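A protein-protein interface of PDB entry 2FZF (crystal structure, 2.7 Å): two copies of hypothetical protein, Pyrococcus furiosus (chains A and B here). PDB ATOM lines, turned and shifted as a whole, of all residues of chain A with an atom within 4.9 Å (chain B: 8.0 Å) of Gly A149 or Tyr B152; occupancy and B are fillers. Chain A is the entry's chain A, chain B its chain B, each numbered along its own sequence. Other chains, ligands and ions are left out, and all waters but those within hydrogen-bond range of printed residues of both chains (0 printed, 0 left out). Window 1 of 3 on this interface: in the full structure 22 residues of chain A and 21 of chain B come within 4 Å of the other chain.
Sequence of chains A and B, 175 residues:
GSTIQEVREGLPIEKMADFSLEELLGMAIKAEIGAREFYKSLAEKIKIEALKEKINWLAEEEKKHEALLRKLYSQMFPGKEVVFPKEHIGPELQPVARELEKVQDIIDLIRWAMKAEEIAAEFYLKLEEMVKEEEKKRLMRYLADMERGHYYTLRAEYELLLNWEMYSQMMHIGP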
ATOM      1  N   ALA A 144      24.956 -11.334  32.198  1.00  0.00           N
ATOM      2  CA  ALA A 144      24.230 -10.600  31.166  1.00  0.00           C
ATOM      3  C   ALA A 144      23.963 -11.435  29.895  1.00  0.00           C
ATOM      4  O   ALA A 144      22.848 -11.421  29.360  1.00  0.00           O
ATOM      5  CB  ALA A 144      24.991  -9.334  30.796  1.00  0.00           C
ATOM      6  N   ASP A 145      24.975 -12.153  29.404  1.00  0.00           N
ATOM      7  CA  ASP A 145      24.799 -12.972  28.203  1.00  0.00           C
ATOM      8  C   ASP A 145      23.846 -14.140  28.429  1.00  0.00           C
ATOM      9  O   ASP A 145      23.055 -14.497  27.545  1.00  0.00           O
ATOM     10  CB  ASP A 145      26.154 -13.461  27.678  1.00  0.00           C
ATOM     11  CG  ASP A 145      26.901 -12.373  26.902  1.00  0.00           C
ATOM     12  OD1 ASP A 145      26.281 -11.319  26.609  1.00  0.00           O
ATOM     13  OD2 ASP A 145      28.093 -12.575  26.580  1.00  0.00           O
ATOM     14  N   MET A 146      23.930 -14.725  29.619  1.00  0.00           N
ATOM     15  CA  MET A 146      23.049 -15.806  30.021  1.00  0.00           C
ATOM     16  C   MET A 146      21.617 -15.257  30.043  1.00  0.00           C
ATOM     17  O   MET A 146      20.697 -15.912  29.583  1.00  0.00           O
ATOM     18  CB  MET A 146      23.418 -16.302  31.428  1.00  0.00           C
ATOM     19  CG  MET A 146      24.571 -17.304  31.494  1.00  0.00           C
ATOM     20  SD  MET A 146      24.361 -18.665  30.327  1.00  0.00           S
ATOM     21  CE  MET A 146      22.847 -19.489  30.929  1.00  0.00           C
ATOM     22  N   GLU A 147      21.436 -14.059  30.595  1.00  0.00           N
ATOM     23  CA  GLU A 147      20.115 -13.444  30.662  1.00  0.00           C
ATOM     24  C   GLU A 147      19.620 -13.087  29.258  1.00  0.00           C
ATOM     25  O   GLU A 147      18.459 -13.306  28.907  1.00  0.00           O
ATOM     26  CB  GLU A 147      20.161 -12.183  31.531  1.00  0.00           C
ATOM     27  CG  GLU A 147      20.300 -12.440  33.030  1.00  0.00           C
ATOM     28  CD  GLU A 147      19.090 -13.149  33.615  1.00  0.00           C
ATOM     29  OE1 GLU A 147      18.948 -14.375  33.417  1.00  0.00           O
ATOM     30  OE2 GLU A 147      18.266 -12.473  34.268  1.00  0.00           O
ATOM     31  N   ARG A 148      20.526 -12.528  28.464  1.00  0.00           N
ATOM     32  CA  ARG A 148      20.233 -12.140  27.096  1.00  0.00           C
ATOM     33  C   ARG A 148      19.741 -13.390  26.355  1.00  0.00           C
ATOM     34  O   ARG A 148      18.805 -13.320  25.565  1.00  0.00           O
ATOM     35  CB  ARG A 148      21.509 -11.588  26.456  1.00  0.00           C
ATOM     36  CG  ARG A 148      21.346 -10.936  25.097  1.00  0.00           C
ATOM     37  CD  ARG A 148      20.606  -9.607  25.163  1.00  0.00           C
ATOM     38  NE  ARG A 148      20.560  -8.981  23.837  1.00  0.00           N
ATOM     39  CZ  ARG A 148      21.627  -8.508  23.190  1.00  0.00           C
ATOM     40  NH1 ARG A 148      22.829  -8.579  23.757  1.00  0.00           N
ATOM     41  NH2 ARG A 148      21.499  -7.993  21.969  1.00  0.00           N
ATOM     42  N   GLY A 149      20.379 -14.530  26.627  1.00  0.00           N
ATOM     43  CA  GLY A 149      19.993 -15.780  25.998  1.00  0.00           C
ATOM     44  C   GLY A 149      18.630 -16.279  26.444  1.00  0.00           C
ATOM     45  O   GLY A 149      17.868 -16.816  25.636  1.00  0.00           O
ATOM     46  N   HIS A 150      18.319 -16.110  27.728  1.00  0.00           N
ATOM     47  CA  HIS A 150      17.028 -16.536  28.260  1.00  0.00           C
ATOM     48  C   HIS A 150      15.933 -15.666  27.629  1.00  0.00           C
ATOM     49  O   HIS A 150      14.819 -16.128  27.393  1.00  0.00           O
ATOM     50  CB  HIS A 150      17.007 -16.409  29.787  1.00  0.00           C
ATOM     51  CG  HIS A 150      18.002 -17.289  30.485  1.00  0.00           C
ATOM     52  ND1 HIS A 150      18.264 -18.586  30.088  1.00  0.00           N
ATOM     53  CD2 HIS A 150      18.781 -17.070  31.573  1.00  0.00           C
ATOM     54  CE1 HIS A 150      19.158 -19.125  30.898  1.00  0.00           C
ATOM     55  NE2 HIS A 150      19.490 -18.226  31.809  1.00  0.00           N
ATOM     56  N   TYR A 151      16.278 -14.412  27.340  1.00  0.00           N
ATOM     57  CA  TYR A 151      15.361 -13.471  26.717  1.00  0.00           C
ATOM     58  C   TYR A 151      14.936 -13.954  25.332  1.00  0.00           C
ATOM     59  O   TYR A 151      13.747 -13.951  24.998  1.00  0.00           O
ATOM     60  CB  TYR A 151      16.006 -12.087  26.586  1.00  0.00           C
ATOM     61  CG  TYR A 151      15.235 -11.145  25.683  1.00  0.00           C
ATOM     62  CD1 TYR A 151      13.972 -10.666  26.054  1.00  0.00           C
ATOM     63  CD2 TYR A 151      15.737 -10.775  24.431  1.00  0.00           C
ATOM     64  CE1 TYR A 151      13.227  -9.845  25.197  1.00  0.00           C
ATOM     65  CE2 TYR A 151      14.998  -9.956  23.567  1.00  0.00           C
ATOM     66  CZ  TYR A 151      13.751  -9.499  23.958  1.00  0.00           C
ATOM     67  OH  TYR A 151      13.017  -8.693  23.115  1.00  0.00           O
ATOM     68  N   TYR A 152      15.902 -14.371  24.519  1.00  0.00           N
ATOM     69  CA  TYR A 152      15.587 -14.844  23.173  1.00  0.00           C
ATOM     70  C   TYR A 152      14.834 -16.176  23.215  1.00  0.00           C
ATOM     71  O   TYR A 152      13.873 -16.387  22.458  1.00  0.00           O
ATOM     72  CB  TYR A 152      16.864 -14.958  22.332  1.00  0.00           C
ATOM     73  CG  TYR A 152      17.355 -13.614  21.812  1.00  0.00           C
ATOM     74  CD1 TYR A 152      16.567 -12.845  20.945  1.00  0.00           C
ATOM     75  CD2 TYR A 152      18.593 -13.098  22.200  1.00  0.00           C
ATOM     76  CE1 TYR A 152      17.002 -11.597  20.480  1.00  0.00           C
ATOM     77  CE2 TYR A 152      19.035 -11.848  21.742  1.00  0.00           C
ATOM     78  CZ  TYR A 152      18.232 -11.109  20.882  1.00  0.00           C
ATOM     79  OH  TYR A 152      18.658  -9.893  20.426  1.00  0.00           O
ATOM     80  N   THR A 153      15.248 -17.068  24.111  1.00  0.00           N
ATOM     81  CA  THR A 153      14.565 -18.347  24.232  1.00  0.00           C
ATOM     82  C   THR A 153      13.107 -18.058  24.582  1.00  0.00           C
ATOM     83  O   THR A 153      12.196 -18.621  23.980  1.00  0.00           O
ATOM     84  CB  THR A 153      15.191 -19.229  25.347  1.00  0.00           C
ATOM     85  OG1 THR A 153      16.582 -19.420  25.079  1.00  0.00           O
ATOM     86  CG2 THR A 153      14.510 -20.586  25.412  1.00  0.00           C
ATOM     87  N   LYS B  54      24.948 -27.881  29.054  1.00  0.00           N
ATOM     88  CA  LYS B  54      24.490 -26.859  28.115  1.00  0.00           C
ATOM     89  C   LYS B  54      24.522 -27.339  26.675  1.00  0.00           C
ATOM     90  O   LYS B  54      23.579 -27.126  25.916  1.00  0.00           O
ATOM     91  CB  LYS B  54      25.338 -25.585  28.234  1.00  0.00           C
ATOM     92  CG  LYS B  54      25.092 -24.785  29.508  1.00  0.00           C
ATOM     93  CD  LYS B  54      25.703 -23.383  29.450  1.00  0.00           C
ATOM     94  CE  LYS B  54      25.465 -22.618  30.757  1.00  0.00           C
ATOM     95  NZ  LYS B  54      26.109 -21.276  30.749  1.00  0.00           N
ATOM     96  N   MET B 114      29.450 -20.825  17.914  1.00  0.00           N
ATOM     97  CA  MET B 114      28.741 -19.545  17.960  1.00  0.00           C
ATOM     98  C   MET B 114      28.842 -18.817  16.646  1.00  0.00           C
ATOM     99  O   MET B 114      27.981 -18.021  16.281  1.00  0.00           O
ATOM    100  CB  MET B 114      29.252 -18.652  19.119  1.00  0.00           C
ATOM    101  CG  MET B 114      30.771 -18.601  19.360  1.00  0.00           C
ATOM    102  SD  MET B 114      31.282 -17.762  20.974  1.00  0.00           S
ATOM    103  CE  MET B 114      31.399 -15.946  20.497  1.00  0.00           C
ATOM    104  N   GLU B 117      26.031 -20.370  14.811  1.00  0.00           N
ATOM    105  CA  GLU B 117      24.733 -19.969  15.364  1.00  0.00           C
ATOM    106  C   GLU B 117      24.401 -18.529  14.945  1.00  0.00           C
ATOM    107  O   GLU B 117      23.259 -18.218  14.620  1.00  0.00           O
ATOM    108  CB  GLU B 117      24.769 -20.088  16.903  1.00  0.00           C
ATOM    109  CG  GLU B 117      24.866 -21.526  17.439  1.00  0.00           C
ATOM    110  CD  GLU B 117      23.601 -22.331  17.184  1.00  0.00           C
ATOM    111  OE1 GLU B 117      23.639 -23.587  17.286  1.00  0.00           O
ATOM    112  OE2 GLU B 117      22.555 -21.701  16.885  1.00  0.00           O
ATOM    113  N   GLU B 118      25.416 -17.667  14.951  1.00  0.00           N
ATOM    114  CA  GLU B 118      25.273 -16.262  14.571  1.00  0.00           C
ATOM    115  C   GLU B 118      24.788 -16.131  13.128  1.00  0.00           C
ATOM    116  O   GLU B 118      23.928 -15.302  12.829  1.00  0.00           O
ATOM    117  CB  GLU B 118      26.613 -15.537  14.721  1.00  0.00           C
ATOM    118  CG  GLU B 118      26.484 -14.028  14.816  1.00  0.00           C
ATOM    119  CD  GLU B 118      27.826 -13.316  14.985  1.00  0.00           C
ATOM    120  OE1 GLU B 118      28.737 -13.901  15.616  1.00  0.00           O
ATOM    121  OE2 GLU B 118      27.962 -12.164  14.506  1.00  0.00           O
ATOM    122  N   ASP B 145      15.176 -16.844  16.867  1.00  0.00           N
ATOM    123  CA  ASP B 145      15.344 -16.573  18.296  1.00  0.00           C
ATOM    124  C   ASP B 145      16.099 -17.683  19.025  1.00  0.00           C
ATOM    125  O   ASP B 145      16.970 -17.415  19.852  1.00  0.00           O
ATOM    126  CB  ASP B 145      13.991 -16.320  18.956  1.00  0.00           C
ATOM    127  CG  ASP B 145      13.406 -14.977  18.557  1.00  0.00           C
ATOM    128  OD1 ASP B 145      14.214 -14.081  18.241  1.00  0.00           O
ATOM    129  OD2 ASP B 145      12.161 -14.814  18.566  1.00  0.00           O
ATOM    130  N   MET B 146      15.767 -18.930  18.726  1.00  0.00           N
ATOM    131  CA  MET B 146      16.456 -20.032  19.360  1.00  0.00           C
ATOM    132  C   MET B 146      17.939 -19.988  18.993  1.00  0.00           C
ATOM    133  O   MET B 146      18.804 -20.154  19.852  1.00  0.00           O
ATOM    134  CB  MET B 146      15.818 -21.350  18.938  1.00  0.00           C
ATOM    135  CG  MET B 146      14.438 -21.574  19.550  1.00  0.00           C
ATOM    136  SD  MET B 146      14.423 -21.433  21.377  1.00  0.00           S
ATOM    137  CE  MET B 146      15.783 -22.539  21.829  1.00  0.00           C
ATOM    138  N   GLU B 147      18.236 -19.747  17.721  1.00  0.00           N
ATOM    139  CA  GLU B 147      19.623 -19.660  17.254  1.00  0.00           C
ATOM    140  C   GLU B 147      20.394 -18.534  17.964  1.00  0.00           C
ATOM    141  O   GLU B 147      21.525 -18.725  18.413  1.00  0.00           O
ATOM    142  CB  GLU B 147      19.637 -19.421  15.734  1.00  0.00           C
ATOM    143  CG  GLU B 147      20.023 -20.630  14.872  1.00  0.00           C
ATOM    144  CD  GLU B 147      19.542 -21.961  15.437  1.00  0.00           C
ATOM    145  OE1 GLU B 147      18.312 -22.170  15.547  1.00  0.00           O
ATOM    146  OE2 GLU B 147      20.404 -22.805  15.773  1.00  0.00           O
ATOM    147  N   ARG B 148      19.778 -17.357  18.057  1.00  0.00           N
ATOM    148  CA  ARG B 148      20.429 -16.227  18.708  1.00  0.00           C
ATOM    149  C   ARG B 148      20.640 -16.605  20.149  1.00  0.00           C
ATOM    150  O   ARG B 148      21.679 -16.307  20.732  1.00  0.00           O
ATOM    151  CB  ARG B 148      19.574 -14.974  18.626  1.00  0.00           C
ATOM    152  CG  ARG B 148      20.378 -13.701  18.806  1.00  0.00           C
ATOM    153  CD  ARG B 148      21.471 -13.565  17.734  1.00  0.00           C
ATOM    154  NE  ARG B 148      22.198 -12.300  17.842  1.00  0.00           N
ATOM    155  CZ  ARG B 148      21.641 -11.101  17.684  1.00  0.00           C
ATOM    156  NH1 ARG B 148      20.348 -11.005  17.404  1.00  0.00           N
ATOM    157  NH2 ARG B 148      22.371  -9.998  17.825  1.00  0.00           N
ATOM    158  N   GLY B 149      19.636 -17.263  20.717  1.00  0.00           N
ATOM    159  CA  GLY B 149      19.723 -17.717  22.087  1.00  0.00           C
ATOM    160  C   GLY B 149      20.945 -18.602  22.287  1.00  0.00           C
ATOM    161  O   GLY B 149      21.654 -18.458  23.287  1.00  0.00           O
ATOM    162  N   HIS B 150      21.209 -19.519  21.356  1.00  0.00           N
ATOM    163  CA  HIS B 150      22.377 -20.382  21.507  1.00  0.00           C
ATOM    164  C   HIS B 150      23.666 -19.582  21.393  1.00  0.00           C
ATOM    165  O   HIS B 150      24.724 -20.010  21.867  1.00  0.00           O
ATOM    166  CB  HIS B 150      22.414 -21.494  20.454  1.00  0.00           C
ATOM    167  CG  HIS B 150      21.232 -22.405  20.488  1.00  0.00           C
ATOM    168  ND1 HIS B 150      20.391 -22.494  21.577  1.00  0.00           N
ATOM    169  CD2 HIS B 150      20.759 -23.275  19.573  1.00  0.00           C
ATOM    170  CE1 HIS B 150      19.448 -23.383  21.328  1.00  0.00           C
ATOM    171  NE2 HIS B 150      19.645 -23.873  20.119  1.00  0.00           N
ATOM    172  N   TYR B 151      23.587 -18.424  20.745  1.00  0.00           N
ATOM    173  CA  TYR B 151      24.771 -17.591  20.576  1.00  0.00           C
ATOM    174  C   TYR B 151      25.280 -17.114  21.930  1.00  0.00           C
ATOM    175  O   TYR B 151      26.444 -17.324  22.275  1.00  0.00           O
ATOM    176  CB  TYR B 151      24.461 -16.375  19.689  1.00  0.00           C
ATOM    177  CG  TYR B 151      25.636 -15.430  19.542  1.00  0.00           C
ATOM    178  CD1 TYR B 151      26.788 -15.824  18.857  1.00  0.00           C
ATOM    179  CD2 TYR B 151      25.623 -14.165  20.142  1.00  0.00           C
ATOM    180  CE1 TYR B 151      27.898 -14.991  18.774  1.00  0.00           C
ATOM    181  CE2 TYR B 151      26.734 -13.321  20.068  1.00  0.00           C
ATOM    182  CZ  TYR B 151      27.870 -13.739  19.382  1.00  0.00           C
ATOM    183  OH  TYR B 151      28.987 -12.927  19.304  1.00  0.00           O
ATOM    184  N   TYR B 152      24.388 -16.478  22.688  1.00  0.00           N
ATOM    185  CA  TYR B 152      24.700 -15.939  24.004  1.00  0.00           C
ATOM    186  C   TYR B 152      25.067 -17.032  24.994  1.00  0.00           C
ATOM    187  O   TYR B 152      26.008 -16.890  25.778  1.00  0.00           O
ATOM    188  CB  TYR B 152      23.516 -15.106  24.495  1.00  0.00           C
ATOM    189  CG  TYR B 152      23.348 -13.841  23.682  1.00  0.00           C
ATOM    190  CD1 TYR B 152      24.269 -12.799  23.787  1.00  0.00           C
ATOM    191  CD2 TYR B 152      22.309 -13.708  22.768  1.00  0.00           C
ATOM    192  CE1 TYR B 152      24.164 -11.648  22.998  1.00  0.00           C
ATOM    193  CE2 TYR B 152      22.194 -12.569  21.973  1.00  0.00           C
ATOM    194  CZ  TYR B 152      23.128 -11.541  22.094  1.00  0.00           C
ATOM    195  OH  TYR B 152      23.015 -10.421  21.305  1.00  0.00           O
ATOM    196  N   THR B 153      24.327 -18.127  24.949  1.00  0.00           N
ATOM    197  CA  THR B 153      24.599 -19.268  25.813  1.00  0.00           C
ATOM    198  C   THR B 153      26.050 -19.727  25.608  1.00  0.00           C
ATOM    199  O   THR B 153      26.791 -19.941  26.570  1.00  0.00           O
ATOM    200  CB  THR B 153      23.669 -20.427  25.462  1.00  0.00           C
ATOM    201  OG1 THR B 153      22.308 -20.020  25.671  1.00  0.00           O
ATOM    202  CG2 THR B 153      23.985 -21.633  26.311  1.00  0.00           C
ATOM    203  N   LEU B 154      26.441 -19.889  24.347  1.00  0.00           N
ATOM    204  CA  LEU B 154      27.792 -20.322  24.022  1.00  0.00           C
ATOM    205  C   LEU B 154      28.795 -19.228  24.369  1.00  0.00           C
ATOM    206  O   LEU B 154      29.856 -19.504  24.934  1.00  0.00           O
ATOM    207  CB  LEU B 154      27.907 -20.665  22.530  1.00  0.00           C
ATOM    208  CG  LEU B 154      27.233 -21.944  21.997  1.00  0.00           C
ATOM    209  CD1 LEU B 154      27.145 -21.884  20.480  1.00  0.00           C
ATOM    210  CD2 LEU B 154      28.008 -23.177  22.457  1.00  0.00           C
ATOM    211  N   ARG B 155      28.463 -17.983  24.037  1.00  0.00           N
ATOM    212  CA  ARG B 155      29.378 -16.894  24.329  1.00  0.00           C
ATOM    213  C   ARG B 155      29.687 -16.864  25.832  1.00  0.00           C
ATOM    214  O   ARG B 155      30.842 -16.668  26.231  1.00  0.00           O
ATOM    215  CB  ARG B 155      28.802 -15.551  23.869  1.00  0.00           C
ATOM    216  CG  ARG B 155      29.873 -14.474  23.735  1.00  0.00           C
ATOM    217  CD  ARG B 155      29.308 -13.079  23.963  1.00  0.00           C
ATOM    218  NE  ARG B 155      28.928 -12.380  22.741  1.00  0.00           N
ATOM    219  CZ  ARG B 155      28.245 -11.238  22.732  1.00  0.00           C
ATOM    220  NH1 ARG B 155      27.923 -10.639  21.585  1.00  0.00           N
ATOM    221  NH2 ARG B 155      27.870 -10.702  23.886  1.00  0.00           N
ATOM    222  N   ALA B 156      28.666 -17.076  26.664  1.00  0.00           N
ATOM    223  CA  ALA B 156      28.859 -17.082  28.114  1.00  0.00           C
ATOM    224  C   ALA B 156      29.959 -18.064  28.535  1.00  0.00           C
ATOM    225  O   ALA B 156      30.959 -17.669  29.133  1.00  0.00           O
ATOM    226  CB  ALA B 156      27.561 -17.433  28.817  1.00  0.00           C
ATOM    227  N   GLU B 157      29.776 -19.341  28.219  1.00  0.00           N
ATOM    228  CA  GLU B 157      30.760 -20.349  28.587  1.00  0.00           C
ATOM    229  C   GLU B 157      32.095 -20.132  27.882  1.00  0.00           C
ATOM    230  O   GLU B 157      33.146 -20.561  28.363  1.00  0.00           O
ATOM    231  CB  GLU B 157      30.221 -21.741  28.270  1.00  0.00           C
ATOM    232  CG  GLU B 157      28.962 -22.096  29.040  1.00  0.00           C
ATOM    233  CD  GLU B 157      29.230 -22.386  30.501  1.00  0.00           C
ATOM    234  OE1 GLU B 157      30.047 -23.288  30.779  1.00  0.00           O
ATOM    235  OE2 GLU B 157      28.626 -21.726  31.372  1.00  0.00           O
ATOM    236  N   TYR B 158      32.056 -19.454  26.743  1.00  0.00           N
ATOM    237  CA  TYR B 158      33.266 -19.186  25.979  1.00  0.00           C
ATOM    238  C   TYR B 158      34.317 -18.436  26.789  1.00  0.00           C
ATOM    239  O   TYR B 158      35.395 -18.969  27.059  1.00  0.00           O
ATOM    240  CB  TYR B 158      32.927 -18.374  24.723  1.00  0.00           C
ATOM    241  CG  TYR B 158      34.142 -17.903  23.946  1.00  0.00           C
ATOM    242  CD1 TYR B 158      35.000 -18.816  23.323  1.00  0.00           C
ATOM    243  CD2 TYR B 158      34.445 -16.547  23.842  1.00  0.00           C
ATOM    244  CE1 TYR B 158      36.129 -18.387  22.616  1.00  0.00           C
ATOM    245  CE2 TYR B 158      35.568 -16.110  23.139  1.00  0.00           C
ATOM    246  CZ  TYR B 158      36.404 -17.034  22.531  1.00  0.00           C
ATOM    247  OH  TYR B 158      37.519 -16.597  21.855  1.00  0.00           O
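Among the printed residues, pairs that only touch across the chains: Asp A145 with Tyr B152, Met A146 with Ala B156, Gly A149 with Tyr B152, Tyr A152 with Asp B145, Tyr A152 with Arg B148, Tyr A152 with Gly B149 and Tyr A152 with Tyr B152.
Asp A145 touches Tyr B152, and with the chains exchanged Tyr A152 touches Asp B145. Arg A148 touches Tyr B152, and with the chains exchanged Tyr A152 touches Arg B148. Gly A149 touches Tyr B152, and with the chains exchanged Tyr A152 touches Gly B149. Tyr A152 touches its own counterpart, Tyr B152. Of the 10 pairs that touch across the chains among the printed residues, 7 have their exchanged pair printed and touching as well.
O of Met A146 lies close to NE2 of His A150 (3.4 Å). The side-chain hydroxyl (OG1) of Thr A153 lies within hydrogen-bond range of the backbone carbonyl oxygen (O) of Gly A149 (3.0 Å). The side-chain carboxylate (OE2) of Glu B157 is in salt-bridge range of the side-chain amino group (NZ) of Lys B54, at 2.6 Å. O of Gly B149 is in hydrogen-bond range of OG1 of Thr B153, 2.9 Å away. The side-chain hydroxyl (OH) of Tyr B151 sits close to the guanidinium group (NH1) of Arg B155.
The side-chain carboxylate (OD1) of Asp A145 is in salt-bridge range of the guanidinium group (NH2) of Arg B155, 3.2 Å away. The side-chain amino group of Lys B54 is in hydrogen-bond range of the side-chain sulfur of Met A146, at 3.2 Å. The guanidinium group (NH2) of Arg A148 is in hydrogen-bond range of the side-chain hydroxyl (OH) of Tyr B152, at 2.9 Å.
Printed residues of chain A that touch a printed residue of chain B: Asp A145, Met A146, Arg A148, Gly A149 and Tyr A152. Hydrophobic or aromatic side chains of chain A within 4 Å of the printed part of chain B: Met A146 and Tyr A152. Printed residues of chain B that touch a printed residue of chain A: Lys B54, Asp B145, Arg B148, Gly B149, Tyr B152, Arg B155 and Ala B156. Hydrophobic or aromatic side chains of chain B that line the printed part of chain A: Tyr B152 and Ala B156. Among the printed residues, Asp or Glu carboxylates within 4 Å of a Lys or Arg side-chain nitrogen of the other chain: Asp A145 with Arg B155 (3.2 Å).
Gly A149 touches one residue of chain B. Tyr B152 touches just these residues of chain A: Asp A145 (3.1 Å), Arg A148 (2.9 Å), Gly A149 (3.8 Å) and Tyr A152 (3.2 Å). Of the printed residues of chain A, Gly B149 touches Tyr A152. Printed residues of chain B within 4 Å of Met A146: Lys B54 and Ala B156. Printed residues of chain A within 4 Å of Lys B54: Met A146. Of the printed residues of chain A, Arg B155 touches Asp A145 (2.9 Å). Glu B117 touches none of the printed residues of chain A. The nearest residue of chain B that does not touch Gly A149 is Gly B149 (4.1 Å). The nearest printed residue of chain B that does not touch Arg A148 is Arg B148 (4.7 Å).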
